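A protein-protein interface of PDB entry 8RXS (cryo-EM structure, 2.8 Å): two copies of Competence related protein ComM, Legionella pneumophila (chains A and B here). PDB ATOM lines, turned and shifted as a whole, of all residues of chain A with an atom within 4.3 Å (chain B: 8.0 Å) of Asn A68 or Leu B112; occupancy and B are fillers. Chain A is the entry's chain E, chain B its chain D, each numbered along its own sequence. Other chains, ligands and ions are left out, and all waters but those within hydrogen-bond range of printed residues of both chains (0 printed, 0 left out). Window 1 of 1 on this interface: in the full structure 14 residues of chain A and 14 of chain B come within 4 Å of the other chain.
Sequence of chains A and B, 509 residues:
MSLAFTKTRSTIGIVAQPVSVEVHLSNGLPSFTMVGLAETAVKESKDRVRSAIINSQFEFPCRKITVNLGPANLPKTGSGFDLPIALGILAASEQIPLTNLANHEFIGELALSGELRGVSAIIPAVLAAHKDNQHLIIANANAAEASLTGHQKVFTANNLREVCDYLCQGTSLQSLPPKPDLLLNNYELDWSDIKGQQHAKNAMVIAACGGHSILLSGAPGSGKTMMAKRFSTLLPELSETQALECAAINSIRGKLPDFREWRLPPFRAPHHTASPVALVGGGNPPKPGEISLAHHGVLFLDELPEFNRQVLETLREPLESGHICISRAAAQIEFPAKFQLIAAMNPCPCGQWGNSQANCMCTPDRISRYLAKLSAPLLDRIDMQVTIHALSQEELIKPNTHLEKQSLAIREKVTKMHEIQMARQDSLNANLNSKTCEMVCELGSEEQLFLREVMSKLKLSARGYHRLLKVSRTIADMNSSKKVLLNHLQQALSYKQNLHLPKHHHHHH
Among the printed residues, pairs that only touch across the chains: Leu A3 with Asn B55, Leu A3 with Leu B112, Leu A3 with Ser B113, Glu A22 with Ala B111, His A24 with Ser B51, His A24 with Leu B112, Val A35 with Glu B44, Val A35 with Asp B47, Val A35 with Arg B48, Thr A66 with Ser B51, Thr A66 with Leu B112, Asn A68 with Arg B48 and Asn A68 with Leu B112.
No position is printed for both chains. Of the 16 pairs that touch across the chains among the printed residues, none has its exchanged pair printed and touching as well.
Of chain B, only Arg B48 and Leu B112 come within 4 Å of Asn A68. Of the printed residues of chain A, Leu B112 touches Leu A3 (3.5 Å), Glu A22 (3.4 Å), His A24 (3.7 Å), Thr A66 (3.3 Å) and Asn A68 (3.3 Å). Of chain B, only Ala B111, Leu B112 and Arg B117 come within 4 Å of Glu A22. Of the printed residues of chain A, Arg B117 touches Glu A22. Of the printed residues of chain B, Val A35 touches Glu B44 (3.5 Å), Asp B47 (3.99 Å) and Arg B48 (3.6 Å). Printed residues of chain B within 4 Å of Thr A66: Ser B51 (3.99 Å) and Leu B112 (3.3 Å). Of the printed residues of chain A, Ser B51 touches His A24 (3.5 Å) and Thr A66 (3.99 Å). Val A67 touches none of the printed residues of chain B. Gly A70 touches none of the printed residues of chain B. The nearest residue of chain B that does not touch Asn A68 is Ala B111 (4.3 Å). The nearest printed residue of chain A that does not touch Leu B112 is Val A23 (4.01 Å).
The side-chain amide oxygen (OD1) of Asn B55 lies within hydrogen-bond range of a ring nitrogen (NE2) of His A24, 2.9 Å away. The backbone NH of Leu B112 lies within hydrogen-bond range of the side-chain carboxylate of Glu A22 (3.4 Å). The side-chain carboxylate (OE2) of Glu A22 is in salt-bridge range of the guanidinium group (NH2) of Arg B117.
Hydrophobic or aromatic side chains of chain B within 4 Å of the printed part of chain A: Ala B111 and Leu B112. Hydrophobic or aromatic side chains of chain A that line the printed part of chain B: Leu A3, His A24 and Val A35. Along chain A the printed residues that touch a printed residue of chain B span positions 3 to 68.
The backbone carbonyl oxygen (O) of Asp B47 lies within hydrogen-bond range of the side-chain hydroxyl (OG) of Ser B51 (3.1 Å). The side-chain amide oxygen of Asn B55 sits close to the backbone carbonyl oxygen of Ser B51, at 3.2 Å. O of Glu B109 sits at hydrogen-bond distance from N of Arg B117, at 2.9 Å. The guanidinium group of Arg B48 is in salt-bridge range of the side-chain carboxylate of Asp B82 (2.6 Å). The backbone carbonyl oxygen (O) of Val A35 is in hydrogen-bond range of the backbone NH (N) of Leu A69, at 2.9 Å. The backbone NH (N) of Asn A68 lies within hydrogen-bond range of the backbone carbonyl oxygen (O) of Glu A22 (2.6 Å).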
ATOM      1  N   LEU A   3     -15.945 -29.909  -8.580  1.00  0.00           N
ATOM      2  CA  LEU A   3     -14.524 -30.235  -8.585  1.00  0.00           C
ATOM      3  C   LEU A   3     -14.292 -31.359  -9.580  1.00  0.00           C
ATOM      4  O   LEU A   3     -14.870 -32.440  -9.435  1.00  0.00           O
ATOM      5  CB  LEU A   3     -14.065 -30.640  -7.184  1.00  0.00           C
ATOM      6  CG  LEU A   3     -12.697 -31.301  -7.027  1.00  0.00           C
ATOM      7  CD1 LEU A   3     -11.601 -30.254  -6.980  1.00  0.00           C
ATOM      8  CD2 LEU A   3     -12.686 -32.147  -5.772  1.00  0.00           C
ATOM      9  N   SER A  20      -1.782 -33.248 -14.021  1.00  0.00           N
ATOM     10  CA  SER A  20      -3.161 -33.480 -13.606  1.00  0.00           C
ATOM     11  C   SER A  20      -3.829 -32.127 -13.397  1.00  0.00           C
ATOM     12  O   SER A  20      -3.695 -31.515 -12.333  1.00  0.00           O
ATOM     13  CB  SER A  20      -3.210 -34.327 -12.337  1.00  0.00           C
ATOM     14  OG  SER A  20      -4.539 -34.708 -12.031  1.00  0.00           O
ATOM     15  N   VAL A  21      -4.549 -31.661 -14.416  1.00  0.00           N
ATOM     16  CA  VAL A  21      -5.285 -30.409 -14.299  1.00  0.00           C
ATOM     17  C   VAL A  21      -6.415 -30.587 -13.298  1.00  0.00           C
ATOM     18  O   VAL A  21      -7.191 -31.549 -13.376  1.00  0.00           O
ATOM     19  CB  VAL A  21      -5.818 -29.969 -15.670  1.00  0.00           C
ATOM     20  CG1 VAL A  21      -6.747 -28.775 -15.522  1.00  0.00           C
ATOM     21  CG2 VAL A  21      -4.663 -29.644 -16.602  1.00  0.00           C
ATOM     22  N   GLU A  22      -6.515 -29.660 -12.350  1.00  0.00           N
ATOM     23  CA  GLU A  22      -7.522 -29.709 -11.300  1.00  0.00           C
ATOM     24  C   GLU A  22      -8.256 -28.380 -11.268  1.00  0.00           C
ATOM     25  O   GLU A  22      -7.625 -27.324 -11.170  1.00  0.00           O
ATOM     26  CB  GLU A  22      -6.884 -30.003  -9.939  1.00  0.00           C
ATOM     27  CG  GLU A  22      -6.033 -31.269  -9.912  1.00  0.00           C
ATOM     28  CD  GLU A  22      -4.899 -31.199  -8.908  1.00  0.00           C
ATOM     29  OE1 GLU A  22      -4.836 -30.218  -8.140  1.00  0.00           O
ATOM     30  OE2 GLU A  22      -4.066 -32.129  -8.889  1.00  0.00           O
ATOM     31  N   VAL A  23      -9.584 -28.433 -11.346  1.00  0.00           N
ATOM     32  CA  VAL A  23     -10.424 -27.245 -11.434  1.00  0.00           C
ATOM     33  C   VAL A  23     -11.422 -27.273 -10.285  1.00  0.00           C
ATOM     34  O   VAL A  23     -12.034 -28.312 -10.015  1.00  0.00           O
ATOM     35  CB  VAL A  23     -11.154 -27.168 -12.785  1.00  0.00           C
ATOM     36  CG1 VAL A  23     -11.973 -25.893 -12.877  1.00  0.00           C
ATOM     37  CG2 VAL A  23     -10.157 -27.252 -13.928  1.00  0.00           C
ATOM     38  N   HIS A  24     -11.584 -26.133  -9.616  1.00  0.00           N
ATOM     39  CA  HIS A  24     -12.526 -26.003  -8.512  1.00  0.00           C
ATOM     40  C   HIS A  24     -13.289 -24.698  -8.663  1.00  0.00           C
ATOM     41  O   HIS A  24     -12.681 -23.643  -8.858  1.00  0.00           O
ATOM     42  CB  HIS A  24     -11.805 -26.038  -7.162  1.00  0.00           C
ATOM     43  CG  HIS A  24     -12.728 -26.022  -5.987  1.00  0.00           C
ATOM     44  ND1 HIS A  24     -12.582 -25.140  -4.937  1.00  0.00           N
ATOM     45  CD2 HIS A  24     -13.807 -26.784  -5.689  1.00  0.00           C
ATOM     46  CE1 HIS A  24     -13.534 -25.357  -4.047  1.00  0.00           C
ATOM     47  NE2 HIS A  24     -14.290 -26.350  -4.480  1.00  0.00           N
ATOM     48  N   VAL A  35      -2.536 -21.998 -11.055  1.00  0.00           N
ATOM     49  CA  VAL A  35      -1.582 -22.421 -10.039  1.00  0.00           C
ATOM     50  C   VAL A  35      -0.716 -23.524 -10.627  1.00  0.00           C
ATOM     51  O   VAL A  35      -1.148 -24.273 -11.507  1.00  0.00           O
ATOM     52  CB  VAL A  35      -2.308 -22.893  -8.756  1.00  0.00           C
ATOM     53  CG1 VAL A  35      -1.412 -23.790  -7.913  1.00  0.00           C
ATOM     54  CG2 VAL A  35      -2.785 -21.698  -7.945  1.00  0.00           C
ATOM     55  N   THR A  66     -10.692 -21.855 -10.222  1.00  0.00           N
ATOM     56  CA  THR A  66      -9.384 -22.083  -9.612  1.00  0.00           C
ATOM     57  C   THR A  66      -8.788 -23.324 -10.256  1.00  0.00           C
ATOM     58  O   THR A  66      -9.212 -24.443  -9.952  1.00  0.00           O
ATOM     59  CB  THR A  66      -9.497 -22.252  -8.101  1.00  0.00           C
ATOM     60  OG1 THR A  66     -10.092 -21.081  -7.529  1.00  0.00           O
ATOM     61  CG2 THR A  66      -8.125 -22.474  -7.483  1.00  0.00           C
ATOM     62  N   VAL A  67      -7.811 -23.130 -11.135  1.00  0.00           N
ATOM     63  CA  VAL A  67      -7.190 -24.217 -11.881  1.00  0.00           C
ATOM     64  C   VAL A  67      -5.809 -24.463 -11.292  1.00  0.00           C
ATOM     65  O   VAL A  67      -4.961 -23.561 -11.274  1.00  0.00           O
ATOM     66  CB  VAL A  67      -7.103 -23.891 -13.379  1.00  0.00           C
ATOM     67  CG1 VAL A  67      -6.556 -25.078 -14.160  1.00  0.00           C
ATOM     68  CG2 VAL A  67      -8.467 -23.490 -13.905  1.00  0.00           C
ATOM     69  N   ASN A  68      -5.585 -25.680 -10.807  1.00  0.00           N
ATOM     70  CA  ASN A  68      -4.290 -26.114 -10.305  1.00  0.00           C
ATOM     71  C   ASN A  68      -3.720 -27.129 -11.284  1.00  0.00           C
ATOM     72  O   ASN A  68      -4.364 -28.142 -11.575  1.00  0.00           O
ATOM     73  CB  ASN A  68      -4.417 -26.717  -8.907  1.00  0.00           C
ATOM     74  CG  ASN A  68      -3.187 -27.494  -8.495  1.00  0.00           C
ATOM     75  OD1 ASN A  68      -2.064 -27.124  -8.832  1.00  0.00           O
ATOM     76  ND2 ASN A  68      -3.390 -28.575  -7.754  1.00  0.00           N
ATOM     77  N   LEU A  69      -2.520 -26.859 -11.789  1.00  0.00           N
ATOM     78  CA  LEU A  69      -1.942 -27.626 -12.889  1.00  0.00           C
ATOM     79  C   LEU A  69      -0.923 -28.617 -12.339  1.00  0.00           C
ATOM     80  O   LEU A  69       0.217 -28.254 -12.043  1.00  0.00           O
ATOM     81  CB  LEU A  69      -1.306 -26.693 -13.912  1.00  0.00           C
ATOM     82  CG  LEU A  69      -2.265 -25.725 -14.603  1.00  0.00           C
ATOM     83  CD1 LEU A  69      -1.494 -24.753 -15.476  1.00  0.00           C
ATOM     84  CD2 LEU A  69      -3.295 -26.479 -15.424  1.00  0.00           C
ATOM     85  N   GLY A  70      -1.342 -29.874 -12.210  1.00  0.00           N
ATOM     86  CA  GLY A  70      -0.442 -30.969 -11.934  1.00  0.00           C
ATOM     87  C   GLY A  70       0.527 -30.684 -10.804  1.00  0.00           C
ATOM     88  O   GLY A  70       0.207 -29.970  -9.848  1.00  0.00           O
ATOM     89  N   GLU B  44       0.782 -19.587  -4.740  1.00  0.00           N
ATOM     90  CA  GLU B  44       0.272 -20.879  -5.174  1.00  0.00           C
ATOM     91  C   GLU B  44      -0.279 -21.698  -4.016  1.00  0.00           C
ATOM     92  O   GLU B  44      -1.361 -22.281  -4.129  1.00  0.00           O
ATOM     93  CB  GLU B  44       1.374 -21.664  -5.895  1.00  0.00           C
ATOM     94  CG  GLU B  44       2.295 -20.815  -6.768  1.00  0.00           C
ATOM     95  CD  GLU B  44       1.571 -20.128  -7.910  1.00  0.00           C
ATOM     96  OE1 GLU B  44       0.323 -20.118  -7.916  1.00  0.00           O
ATOM     97  OE2 GLU B  44       2.256 -19.592  -8.808  1.00  0.00           O
ATOM     98  N   ASP B  47      -4.142 -20.823  -2.836  1.00  0.00           N
ATOM     99  CA  ASP B  47      -5.346 -21.358  -3.460  1.00  0.00           C
ATOM    100  C   ASP B  47      -5.461 -22.859  -3.240  1.00  0.00           C
ATOM    101  O   ASP B  47      -6.561 -23.374  -3.013  1.00  0.00           O
ATOM    102  CB  ASP B  47      -5.343 -21.031  -4.952  1.00  0.00           C
ATOM    103  CG  ASP B  47      -5.447 -19.544  -5.220  1.00  0.00           C
ATOM    104  OD1 ASP B  47      -6.562 -18.994  -5.113  1.00  0.00           O
ATOM    105  OD2 ASP B  47      -4.409 -18.923  -5.534  1.00  0.00           O
ATOM    106  N   ARG B  48      -4.341 -23.578  -3.309  1.00  0.00           N
ATOM    107  CA  ARG B  48      -4.383 -25.013  -3.063  1.00  0.00           C
ATOM    108  C   ARG B  48      -4.876 -25.300  -1.653  1.00  0.00           C
ATOM    109  O   ARG B  48      -5.738 -26.160  -1.446  1.00  0.00           O
ATOM    110  CB  ARG B  48      -3.003 -25.630  -3.283  1.00  0.00           C
ATOM    111  CG  ARG B  48      -2.542 -25.604  -4.727  1.00  0.00           C
ATOM    112  CD  ARG B  48      -1.547 -26.714  -5.003  1.00  0.00           C
ATOM    113  NE  ARG B  48      -0.386 -26.641  -4.125  1.00  0.00           N
ATOM    114  CZ  ARG B  48       0.708 -25.937  -4.380  1.00  0.00           C
ATOM    115  NH1 ARG B  48       0.826 -25.214  -5.482  1.00  0.00           N
ATOM    116  NH2 ARG B  48       1.710 -25.959  -3.508  1.00  0.00           N
ATOM    117  N   VAL B  49      -4.351 -24.572  -0.665  1.00  0.00           N
ATOM    118  CA  VAL B  49      -4.781 -24.775   0.712  1.00  0.00           C
ATOM    119  C   VAL B  49      -6.256 -24.428   0.863  1.00  0.00           C
ATOM    120  O   VAL B  49      -7.017 -25.161   1.505  1.00  0.00           O
ATOM    121  CB  VAL B  49      -3.907 -23.950   1.672  1.00  0.00           C
ATOM    122  CG1 VAL B  49      -4.477 -23.997   3.079  1.00  0.00           C
ATOM    123  CG2 VAL B  49      -2.474 -24.457   1.648  1.00  0.00           C
ATOM    124  N   ARG B  50      -6.683 -23.309   0.276  1.00  0.00           N
ATOM    125  CA  ARG B  50      -8.082 -22.912   0.387  1.00  0.00           C
ATOM    126  C   ARG B  50      -9.003 -23.992  -0.167  1.00  0.00           C
ATOM    127  O   ARG B  50      -9.959 -24.414   0.495  1.00  0.00           O
ATOM    128  CB  ARG B  50      -8.305 -21.589  -0.346  1.00  0.00           C
ATOM    129  CG  ARG B  50      -9.757 -21.151  -0.397  1.00  0.00           C
ATOM    130  CD  ARG B  50      -9.905 -19.790  -1.051  1.00  0.00           C
ATOM    131  NE  ARG B  50     -11.299 -19.367  -1.107  1.00  0.00           N
ATOM    132  CZ  ARG B  50     -12.219 -19.918  -1.887  1.00  0.00           C
ATOM    133  NH1 ARG B  50     -11.926 -20.912  -2.709  1.00  0.00           N
ATOM    134  NH2 ARG B  50     -13.465 -19.458  -1.843  1.00  0.00           N
ATOM    135  N   SER B  51      -8.724 -24.455  -1.387  1.00  0.00           N
ATOM    136  CA  SER B  51      -9.588 -25.448  -2.013  1.00  0.00           C
ATOM    137  C   SER B  51      -9.548 -26.770  -1.260  1.00  0.00           C
ATOM    138  O   SER B  51     -10.585 -27.421  -1.086  1.00  0.00           O
ATOM    139  CB  SER B  51      -9.182 -25.647  -3.471  1.00  0.00           C
ATOM    140  OG  SER B  51      -9.230 -24.421  -4.180  1.00  0.00           O
ATOM    141  N   ALA B  52      -8.366 -27.188  -0.802  1.00  0.00           N
ATOM    142  CA  ALA B  52      -8.268 -28.445  -0.073  1.00  0.00           C
ATOM    143  C   ALA B  52      -9.061 -28.388   1.223  1.00  0.00           C
ATOM    144  O   ALA B  52      -9.735 -29.356   1.591  1.00  0.00           O
ATOM    145  CB  ALA B  52      -6.804 -28.775   0.208  1.00  0.00           C
ATOM    146  N   ILE B  53      -8.997 -27.259   1.930  1.00  0.00           N
ATOM    147  CA  ILE B  53      -9.761 -27.125   3.166  1.00  0.00           C
ATOM    148  C   ILE B  53     -11.253 -27.132   2.865  1.00  0.00           C
ATOM    149  O   ILE B  53     -12.031 -27.825   3.530  1.00  0.00           O
ATOM    150  CB  ILE B  53      -9.342 -25.850   3.917  1.00  0.00           C
ATOM    151  CG1 ILE B  53      -7.894 -25.971   4.392  1.00  0.00           C
ATOM    152  CG2 ILE B  53     -10.264 -25.610   5.101  1.00  0.00           C
ATOM    153  CD1 ILE B  53      -7.304 -24.673   4.889  1.00  0.00           C
ATOM    154  N   ILE B  54     -11.676 -26.378   1.848  1.00  0.00           N
ATOM    155  CA  ILE B  54     -13.105 -26.283   1.556  1.00  0.00           C
ATOM    156  C   ILE B  54     -13.662 -27.644   1.160  1.00  0.00           C
ATOM    157  O   ILE B  54     -14.741 -28.045   1.612  1.00  0.00           O
ATOM    158  CB  ILE B  54     -13.359 -25.230   0.462  1.00  0.00           C
ATOM    159  CG1 ILE B  54     -13.330 -23.827   1.070  1.00  0.00           C
ATOM    160  CG2 ILE B  54     -14.698 -25.485  -0.221  1.00  0.00           C
ATOM    161  CD1 ILE B  54     -13.359 -22.713   0.045  1.00  0.00           C
ATOM    162  N   ASN B  55     -12.941 -28.377   0.311  1.00  0.00           N
ATOM    163  CA  ASN B  55     -13.463 -29.625  -0.230  1.00  0.00           C
ATOM    164  C   ASN B  55     -13.465 -30.758   0.786  1.00  0.00           C
ATOM    165  O   ASN B  55     -14.192 -31.739   0.592  1.00  0.00           O
ATOM    166  CB  ASN B  55     -12.652 -30.041  -1.456  1.00  0.00           C
ATOM    167  CG  ASN B  55     -13.218 -29.476  -2.742  1.00  0.00           C
ATOM    168  OD1 ASN B  55     -12.688 -28.513  -3.296  1.00  0.00           O
ATOM    169  ND2 ASN B  55     -14.303 -30.070  -3.221  1.00  0.00           N
ATOM    170  N   SER B  56     -12.680 -30.653   1.856  1.00  0.00           N
ATOM    171  CA  SER B  56     -12.647 -31.669   2.897  1.00  0.00           C
ATOM    172  C   SER B  56     -13.716 -31.448   3.963  1.00  0.00           C
ATOM    173  O   SER B  56     -13.587 -31.969   5.076  1.00  0.00           O
ATOM    174  CB  SER B  56     -11.261 -31.712   3.546  1.00  0.00           C
ATOM    175  OG  SER B  56     -10.299 -32.234   2.648  1.00  0.00           O
ATOM    176  N   ASP B  82       1.901 -26.946   2.070  1.00  0.00           N
ATOM    177  CA  ASP B  82       0.445 -26.859   2.034  1.00  0.00           C
ATOM    178  C   ASP B  82      -0.192 -27.576   3.218  1.00  0.00           C
ATOM    179  O   ASP B  82      -1.164 -27.077   3.793  1.00  0.00           O
ATOM    180  CB  ASP B  82      -0.081 -27.431   0.719  1.00  0.00           C
ATOM    181  CG  ASP B  82       0.544 -26.775  -0.492  1.00  0.00           C
ATOM    182  OD1 ASP B  82       1.400 -25.887  -0.310  1.00  0.00           O
ATOM    183  OD2 ASP B  82       0.176 -27.143  -1.628  1.00  0.00           O
ATOM    184  N   GLU B 109       1.979 -31.818  -0.041  1.00  0.00           N
ATOM    185  CA  GLU B 109       1.323 -30.813  -0.862  1.00  0.00           C
ATOM    186  C   GLU B 109      -0.084 -31.284  -1.196  1.00  0.00           C
ATOM    187  O   GLU B 109      -0.294 -32.454  -1.530  1.00  0.00           O
ATOM    188  CB  GLU B 109       2.123 -30.537  -2.141  1.00  0.00           C
ATOM    189  CG  GLU B 109       1.862 -31.506  -3.282  1.00  0.00           C
ATOM    190  CD  GLU B 109       2.698 -31.193  -4.508  1.00  0.00           C
ATOM    191  OE1 GLU B 109       3.934 -31.364  -4.446  1.00  0.00           O
ATOM    192  OE2 GLU B 109       2.119 -30.778  -5.534  1.00  0.00           O
ATOM    193  N   LEU B 110      -1.043 -30.370  -1.105  1.00  0.00           N
ATOM    194  CA  LEU B 110      -2.456 -30.694  -1.235  1.00  0.00           C
ATOM    195  C   LEU B 110      -2.943 -30.389  -2.644  1.00  0.00           C
ATOM    196  O   LEU B 110      -2.654 -29.319  -3.189  1.00  0.00           O
ATOM    197  CB  LEU B 110      -3.286 -29.904  -0.223  1.00  0.00           C
ATOM    198  CG  LEU B 110      -3.043 -30.227   1.249  1.00  0.00           C
ATOM    199  CD1 LEU B 110      -3.663 -29.158   2.129  1.00  0.00           C
ATOM    200  CD2 LEU B 110      -3.610 -31.589   1.591  1.00  0.00           C
ATOM    201  N   ALA B 111      -3.677 -31.331  -3.227  1.00  0.00           N
ATOM    202  CA  ALA B 111      -4.399 -31.072  -4.461  1.00  0.00           C
ATOM    203  C   ALA B 111      -5.667 -30.282  -4.146  1.00  0.00           C
ATOM    204  O   ALA B 111      -5.916 -29.885  -3.004  1.00  0.00           O
ATOM    205  CB  ALA B 111      -4.724 -32.382  -5.172  1.00  0.00           C
ATOM    206  N   LEU B 112      -6.487 -30.048  -5.166  1.00  0.00           N
ATOM    207  CA  LEU B 112      -7.732 -29.321  -4.965  1.00  0.00           C
ATOM    208  C   LEU B 112      -8.835 -30.192  -4.381  1.00  0.00           C
ATOM    209  O   LEU B 112      -9.869 -29.657  -3.969  1.00  0.00           O
ATOM    210  CB  LEU B 112      -8.208 -28.717  -6.286  1.00  0.00           C
ATOM    211  CG  LEU B 112      -7.859 -27.244  -6.488  1.00  0.00           C
ATOM    212  CD1 LEU B 112      -6.382 -27.005  -6.234  1.00  0.00           C
ATOM    213  CD2 LEU B 112      -8.240 -26.800  -7.884  1.00  0.00           C
ATOM    214  N   SER B 113      -8.644 -31.505  -4.336  1.00  0.00           N
ATOM    215  CA  SER B 113      -9.628 -32.418  -3.772  1.00  0.00           C
ATOM    216  C   SER B 113      -9.401 -32.685  -2.293  1.00  0.00           C
ATOM    217  O   SER B 113     -10.186 -33.417  -1.683  1.00  0.00           O
ATOM    218  CB  SER B 113      -9.602 -33.748  -4.530  1.00  0.00           C
ATOM    219  OG  SER B 113      -8.281 -34.249  -4.628  1.00  0.00           O
ATOM    220  N   GLY B 114      -8.356 -32.111  -1.702  1.00  0.00           N
ATOM    221  CA  GLY B 114      -7.934 -32.473  -0.370  1.00  0.00           C
ATOM    222  C   GLY B 114      -6.969 -33.635  -0.324  1.00  0.00           C
ATOM    223  O   GLY B 114      -6.466 -33.959   0.758  1.00  0.00           O
ATOM    224  N   GLU B 115      -6.699 -34.271  -1.460  1.00  0.00           N
ATOM    225  CA  GLU B 115      -5.751 -35.370  -1.506  1.00  0.00           C
ATOM    226  C   GLU B 115      -4.333 -34.854  -1.288  1.00  0.00           C
ATOM    227  O   GLU B 115      -4.027 -33.680  -1.510  1.00  0.00           O
ATOM    228  CB  GLU B 115      -5.843 -36.098  -2.845  1.00  0.00           C
ATOM    229  CG  GLU B 115      -7.214 -36.684  -3.140  1.00  0.00           C
ATOM    230  CD  GLU B 115      -7.425 -38.033  -2.482  1.00  0.00           C
ATOM    231  OE1 GLU B 115      -6.618 -38.951  -2.734  1.00  0.00           O
ATOM    232  OE2 GLU B 115      -8.397 -38.175  -1.711  1.00  0.00           O
ATOM    233  N   LEU B 116      -3.462 -35.755  -0.845  1.00  0.00           N
ATOM    234  CA  LEU B 116      -2.076 -35.431  -0.528  1.00  0.00           C
ATOM    235  C   LEU B 116      -1.171 -36.065  -1.577  1.00  0.00           C
ATOM    236  O   LEU B 116      -1.062 -37.294  -1.649  1.00  0.00           O
ATOM    237  CB  LEU B 116      -1.715 -35.919   0.872  1.00  0.00           C
ATOM    238  CG  LEU B 116      -2.142 -35.012   2.026  1.00  0.00           C
ATOM    239  CD1 LEU B 116      -2.145 -35.779   3.333  1.00  0.00           C
ATOM    240  CD2 LEU B 116      -1.222 -33.810   2.118  1.00  0.00           C
ATOM    241  N   ARG B 117      -0.525 -35.230  -2.386  1.00  0.00           N
ATOM    242  CA  ARG B 117       0.482 -35.707  -3.316  1.00  0.00           C
ATOM    243  C   ARG B 117       1.813 -35.877  -2.585  1.00  0.00           C
ATOM    244  O   ARG B 117       1.933 -35.601  -1.390  1.00  0.00           O
ATOM    245  CB  ARG B 117       0.619 -34.747  -4.496  1.00  0.00           C
ATOM    246  CG  ARG B 117      -0.702 -34.314  -5.112  1.00  0.00           C
ATOM    247  CD  ARG B 117      -1.490 -35.499  -5.638  1.00  0.00           C
ATOM    248  NE  ARG B 117      -2.566 -35.083  -6.531  1.00  0.00           N
ATOM    249  CZ  ARG B 117      -3.594 -35.846  -6.874  1.00  0.00           C
ATOM    250  NH1 ARG B 117      -3.723 -37.080  -6.419  1.00  0.00           N
ATOM    251  NH2 ARG B 117      -4.517 -35.357  -7.697  1.00  0.00           N
